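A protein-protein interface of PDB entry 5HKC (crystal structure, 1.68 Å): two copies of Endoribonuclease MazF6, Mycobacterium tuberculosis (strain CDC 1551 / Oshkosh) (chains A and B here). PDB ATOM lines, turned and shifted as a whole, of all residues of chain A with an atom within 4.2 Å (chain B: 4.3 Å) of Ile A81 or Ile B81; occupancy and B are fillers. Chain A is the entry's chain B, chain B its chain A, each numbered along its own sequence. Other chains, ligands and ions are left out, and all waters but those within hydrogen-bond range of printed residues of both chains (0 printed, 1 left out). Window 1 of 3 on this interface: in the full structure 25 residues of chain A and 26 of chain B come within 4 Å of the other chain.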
ATOM      1  N   ILE A  44      17.330 -10.840  -5.479  1.00  0.00           N
ATOM      2  CA  ILE A  44      16.287  -9.841  -5.281  1.00  0.00           C
ATOM      3  C   ILE A  44      16.243  -8.916  -6.487  1.00  0.00           C
ATOM      4  O   ILE A  44      17.282  -8.490  -6.998  1.00  0.00           O
ATOM      5  CB  ILE A  44      16.550  -9.004  -4.008  1.00  0.00           C
ATOM      6  CG1 ILE A  44      16.653  -9.902  -2.771  1.00  0.00           C
ATOM      7  CG2 ILE A  44      15.450  -7.966  -3.813  1.00  0.00           C
ATOM      8  CD1 ILE A  44      17.188  -9.170  -1.523  1.00  0.00           C
ATOM      9  N   ALA A  45      15.034  -8.597  -6.939  1.00  0.00           N
ATOM     10  CA  ALA A  45      14.865  -7.776  -8.130  1.00  0.00           C
ATOM     11  C   ALA A  45      13.661  -6.877  -8.000  1.00  0.00           C
ATOM     12  O   ALA A  45      12.775  -7.132  -7.188  1.00  0.00           O
ATOM     13  CB  ALA A  45      14.720  -8.665  -9.376  1.00  0.00           C
ATOM     14  N   VAL A  78       9.898   0.524  -8.137  1.00  0.00           N
ATOM     15  CA  VAL A  78      10.682   0.317  -6.933  1.00  0.00           C
ATOM     16  C   VAL A  78       9.821  -0.100  -5.750  1.00  0.00           C
ATOM     17  O   VAL A  78      10.361  -0.451  -4.701  1.00  0.00           O
ATOM     18  CB  VAL A  78      11.493   1.589  -6.558  1.00  0.00           C
ATOM     19  CG1 VAL A  78      12.590   1.809  -7.577  1.00  0.00           C
ATOM     20  CG2 VAL A  78      10.591   2.798  -6.474  1.00  0.00           C
ATOM     21  N   THR A  79       8.496  -0.085  -5.911  1.00  0.00           N
ATOM     22  CA  THR A  79       7.606  -0.603  -4.877  1.00  0.00           C
ATOM     23  C   THR A  79       7.280  -2.088  -5.073  1.00  0.00           C
ATOM     24  O   THR A  79       6.575  -2.676  -4.276  1.00  0.00           O
ATOM     25  CB  THR A  79       6.266   0.158  -4.805  1.00  0.00           C
ATOM     26  OG1 THR A  79       5.530  -0.059  -6.014  1.00  0.00           O
ATOM     27  CG2 THR A  79       6.506   1.651  -4.596  1.00  0.00           C
ATOM     28  N   ALA A  80       7.820  -2.684  -6.127  1.00  0.00           N
ATOM     29  CA  ALA A  80       7.532  -4.072  -6.425  1.00  0.00           C
ATOM     30  C   ALA A  80       8.826  -4.869  -6.373  1.00  0.00           C
ATOM     31  O   ALA A  80       9.520  -5.039  -7.384  1.00  0.00           O
ATOM     32  CB  ALA A  80       6.869  -4.207  -7.796  1.00  0.00           C
ATOM     33  N   ILE A  81       9.148  -5.351  -5.183  1.00  0.00           N
ATOM     34  CA  ILE A  81      10.412  -6.037  -4.961  1.00  0.00           C
ATOM     35  C   ILE A  81      10.123  -7.513  -4.744  1.00  0.00           C
ATOM     36  O   ILE A  81       9.241  -7.881  -3.950  1.00  0.00           O
ATOM     37  CB  ILE A  81      11.163  -5.439  -3.759  1.00  0.00           C
ATOM     38  CG1 ILE A  81      11.473  -3.956  -4.030  1.00  0.00           C
ATOM     39  CG2 ILE A  81      12.452  -6.205  -3.498  1.00  0.00           C
ATOM     40  CD1 ILE A  81      12.284  -3.275  -2.954  1.00  0.00           C
ATOM     41  N   VAL A  82      10.840  -8.352  -5.484  1.00  0.00           N
ATOM     42  CA  VAL A  82      10.614  -9.784  -5.418  1.00  0.00           C
ATOM     43  C   VAL A  82      11.929 -10.508  -5.172  1.00  0.00           C
ATOM     44  O   VAL A  82      13.010 -10.014  -5.536  1.00  0.00           O
ATOM     45  CB  VAL A  82       9.939 -10.314  -6.708  1.00  0.00           C
ATOM     46  CG1 VAL A  82       8.538  -9.689  -6.847  1.00  0.00           C
ATOM     47  CG2 VAL A  82      10.794 -10.046  -7.947  1.00  0.00           C
ATOM     48  N   THR A  83      11.826 -11.675  -4.540  1.00  0.00           N
ATOM     49  CA  THR A  83      12.972 -12.537  -4.339  1.00  0.00           C
ATOM     50  C   THR A  83      12.722 -13.784  -5.165  1.00  0.00           C
ATOM     51  O   THR A  83      11.748 -14.486  -4.933  1.00  0.00           O
ATOM     52  CB  THR A  83      13.159 -12.889  -2.864  1.00  0.00           C
ATOM     53  OG1 THR A  83      13.322 -11.684  -2.109  1.00  0.00           O
ATOM     54  CG2 THR A  83      14.375 -13.802  -2.664  1.00  0.00           C
ATOM     55  N   LEU A 108      14.875   3.213  -4.541  1.00  0.00           N
ATOM     56  CA  LEU A 108      14.872   2.149  -3.538  1.00  0.00           C
ATOM     57  C   LEU A 108      15.121   2.675  -2.130  1.00  0.00           C
ATOM     58  O   LEU A 108      14.474   2.255  -1.175  1.00  0.00           O
ATOM     59  CB  LEU A 108      15.923   1.109  -3.891  1.00  0.00           C
ATOM     60  CG  LEU A 108      15.666   0.343  -5.188  1.00  0.00           C
ATOM     61  CD1 LEU A 108      16.925  -0.424  -5.589  1.00  0.00           C
ATOM     62  CD2 LEU A 108      14.470  -0.621  -5.047  1.00  0.00           C
ATOM     63  N   ILE B  30       9.463  -3.201   5.949  1.00  0.00           N
ATOM     64  CA  ILE B  30      10.614  -2.343   5.694  1.00  0.00           C
ATOM     65  C   ILE B  30      10.272  -1.191   4.750  1.00  0.00           C
ATOM     66  O   ILE B  30      11.085  -0.313   4.512  1.00  0.00           O
ATOM     67  CB  ILE B  30      11.817  -3.148   5.129  1.00  0.00           C
ATOM     68  CG1 ILE B  30      11.456  -3.908   3.843  1.00  0.00           C
ATOM     69  CG2 ILE B  30      12.320  -4.140   6.171  1.00  0.00           C
ATOM     70  CD1 ILE B  30      12.678  -4.493   3.143  1.00  0.00           C
ATOM     71  N   ILE B  44       6.294  -3.676   1.420  1.00  0.00           N
ATOM     72  CA  ILE B  44       7.484  -4.504   1.289  1.00  0.00           C
ATOM     73  C   ILE B  44       7.959  -4.954   2.668  1.00  0.00           C
ATOM     74  O   ILE B  44       7.967  -4.168   3.622  1.00  0.00           O
ATOM     75  CB  ILE B  44       8.606  -3.739   0.566  1.00  0.00           C
ATOM     76  CG1 ILE B  44       8.106  -3.222  -0.790  1.00  0.00           C
ATOM     77  CG2 ILE B  44       9.836  -4.614   0.398  1.00  0.00           C
ATOM     78  CD1 ILE B  44       9.014  -2.223  -1.434  1.00  0.00           C
ATOM     79  N   ALA B  45       8.344  -6.219   2.779  1.00  0.00           N
ATOM     80  CA  ALA B  45       8.748  -6.734   4.081  1.00  0.00           C
ATOM     81  C   ALA B  45       9.890  -7.715   3.945  1.00  0.00           C
ATOM     82  O   ALA B  45      10.069  -8.326   2.896  1.00  0.00           O
ATOM     83  CB  ALA B  45       7.560  -7.414   4.774  1.00  0.00           C
ATOM     84  N   VAL B  78      17.521 -10.676   5.486  1.00  0.00           N
ATOM     85  CA  VAL B  78      17.488  -9.523   4.583  1.00  0.00           C
ATOM     86  C   VAL B  78      17.725  -9.928   3.136  1.00  0.00           C
ATOM     87  O   VAL B  78      17.591  -9.105   2.236  1.00  0.00           O
ATOM     88  CB  VAL B  78      18.521  -8.443   4.989  1.00  0.00           C
ATOM     89  CG1 VAL B  78      18.119  -7.815   6.318  1.00  0.00           C
ATOM     90  CG2 VAL B  78      19.905  -9.037   5.081  1.00  0.00           C
ATOM     91  N   THR B  79      18.052 -11.199   2.899  1.00  0.00           N
ATOM     92  CA  THR B  79      18.149 -11.685   1.532  1.00  0.00           C
ATOM     93  C   THR B  79      16.796 -12.206   1.045  1.00  0.00           C
ATOM     94  O   THR B  79      16.673 -12.652  -0.100  1.00  0.00           O
ATOM     95  CB  THR B  79      19.191 -12.822   1.382  1.00  0.00           C
ATOM     96  OG1 THR B  79      18.739 -13.975   2.109  1.00  0.00           O
ATOM     97  CG2 THR B  79      20.557 -12.387   1.890  1.00  0.00           C
ATOM     98  N   ALA B  80      15.787 -12.142   1.911  1.00  0.00           N
ATOM     99  CA  ALA B  80      14.451 -12.649   1.591  1.00  0.00           C
ATOM    100  C   ALA B  80      13.395 -11.554   1.728  1.00  0.00           C
ATOM    101  O   ALA B  80      12.832 -11.342   2.802  1.00  0.00           O
ATOM    102  CB  ALA B  80      14.105 -13.839   2.478  1.00  0.00           C
ATOM    103  N   ILE B  81      13.150 -10.849   0.632  1.00  0.00           N
ATOM    104  CA  ILE B  81      12.258  -9.685   0.627  1.00  0.00           C
ATOM    105  C   ILE B  81      11.004  -9.989  -0.190  1.00  0.00           C
ATOM    106  O   ILE B  81      11.100 -10.561  -1.274  1.00  0.00           O
ATOM    107  CB  ILE B  81      13.005  -8.450   0.067  1.00  0.00           C
ATOM    108  CG1 ILE B  81      14.252  -8.165   0.920  1.00  0.00           C
ATOM    109  CG2 ILE B  81      12.086  -7.251  -0.005  1.00  0.00           C
ATOM    110  CD1 ILE B  81      15.011  -6.885   0.513  1.00  0.00           C
ATOM    111  N   VAL B  82       9.837  -9.647   0.352  1.00  0.00           N
ATOM    112  CA  VAL B  82       8.583  -9.912  -0.340  1.00  0.00           C
ATOM    113  C   VAL B  82       7.768  -8.643  -0.449  1.00  0.00           C
ATOM    114  O   VAL B  82       7.904  -7.731   0.372  1.00  0.00           O
ATOM    115  CB  VAL B  82       7.741 -10.979   0.377  1.00  0.00           C
ATOM    116  CG1 VAL B  82       8.434 -12.323   0.331  1.00  0.00           C
ATOM    117  CG2 VAL B  82       7.434 -10.546   1.812  1.00  0.00           C
ATOM    118  N   THR B  83       6.936  -8.586  -1.485  1.00  0.00           N
ATOM    119  CA  THR B  83       5.982  -7.507  -1.624  1.00  0.00           C
ATOM    120  C   THR B  83       4.610  -8.134  -1.509  1.00  0.00           C
ATOM    121  O   THR B  83       4.262  -9.032  -2.280  1.00  0.00           O
ATOM    122  CB  THR B  83       6.162  -6.759  -2.955  1.00  0.00           C
ATOM    123  OG1 THR B  83       7.468  -6.176  -2.981  1.00  0.00           O
ATOM    124  CG2 THR B  83       5.129  -5.662  -3.105  1.00  0.00           C
ATOM    125  N   LEU B 108      20.088  -4.321   4.885  1.00  0.00           N
ATOM    126  CA  LEU B 108      19.431  -4.070   3.609  1.00  0.00           C
ATOM    127  C   LEU B 108      20.340  -3.272   2.667  1.00  0.00           C
ATOM    128  O   LEU B 108      20.409  -3.557   1.475  1.00  0.00           O
ATOM    129  CB  LEU B 108      18.123  -3.307   3.823  1.00  0.00           C
ATOM    130  CG  LEU B 108      17.034  -4.062   4.571  1.00  0.00           C
ATOM    131  CD1 LEU B 108      15.908  -3.100   4.962  1.00  0.00           C
ATOM    132  CD2 LEU B 108      16.509  -5.223   3.733  1.00  0.00           C
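The backbone carbonyl oxygen of Ile A81 is in hydrogen-bond range of the side-chain hydroxyl of Thr B83 (2.6 Å).
The side-chain hydroxyl (OG1) of Thr A83 is in hydrogen-bond range of the backbone carbonyl oxygen (O) of Ile B81 (2.6 Å).
Ile A44 touches Val B78, and with the chains exchanged Val A78 touches Ile B44.
Ile A44 touches Thr B79, and with the chains exchanged Thr A79 touches Ile B44.
Ile A44 touches Ile B81, and with the chains exchanged Ile A81 touches Ile B44.
Ile A81 touches its own counterpart, Ile B81.
9 positions are printed for both chains.
Among the printed residues, merely in contact across the chains: Thr A79 with Thr B83 (3.5 Å), Thr A83 with Thr B79 (3.6 Å), Ile A81 with Ile B81 (3.7 Å), Ile A44 with Ile B81 (3.8 Å), Ile A81 with Ile B44 (3.8 Å), Thr A79 with Ile B44 (3.8 Å), Ile A44 with Val B78 (3.8 Å), Ile A44 with Thr B79 (3.8 Å), Thr A83 with Ala B80 (3.8 Å), Ile A81 with Val B82 (3.9 Å), Ala A80 with Thr B83 (3.9 Å), Val A78 with Ile B44 (3.95 Å) and Val A82 with Ile B81 (3.99 Å).
Hydrophobic or aromatic side chains of chain B within 4 Å of the printed part of chain A: Ile B44 and Ile B81.
Of the 9 printed residues of chain A, 7 touch a printed residue of chain B.
Printed residues of chain A that touch a printed residue of chain B: Ile A44, Val A78, Thr A79, Ala A80, Ile A81, Val A82 and Thr A83.
Hydrophobic or aromatic side chains of chain A that line the printed part of chain B: Ile A44 and Ile A81.
Among the printed residues, no Asp or Glu carboxylate lies within 4 Å of a Lys or Arg side-chain nitrogen of the other chain.
The backbone carbonyl oxygen (O) of Ala B45 lies within hydrogen-bond range of the backbone NH (N) of Val B82, 2.9 Å away.
The backbone NH of Ile B30 lies within hydrogen-bond range of the backbone carbonyl oxygen of Ile B44.
The backbone NH (N) of Ala A45 is in hydrogen-bond range of the backbone carbonyl oxygen (O) of Val A82, at 2.8 Å.
Of chain B, only Ile B44, Ile B81, Val B82 and Thr B83 come within 4 Å of Ile A81.
Of the printed residues of chain A, Ile B81 touches Ile A44, Ile A81, Val A82 and Thr A83.
Of the printed residues of chain B, Thr A79 touches Ile B44 (3.8 Å) and Thr B83 (3.5 Å).
Printed residues of chain B within 4 Å of Val A78: Ile B44.
Printed residues of chain B within 4 Å of Thr A83: Thr B79 (3.6 Å), Ala B80 (3.8 Å) and Ile B81 (2.6 Å).
Of the printed residues of chain A, Ile B44 touches Val A78, Thr A79 and Ile A81.
Of the printed residues of chain B, Val A82 touches Ile B81.
Ile B30 touches none of the printed residues of chain A.
The nearest printed residue of chain B that does not touch Ile A81 is Ile B30 (6.2 Å).
The nearest printed residue of chain A that does not touch Ile B81 is Ala A45 (7.0 Å).
The nearest printed residue of chain A that does not touch Val B78 is Thr A83 (6.6 Å).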
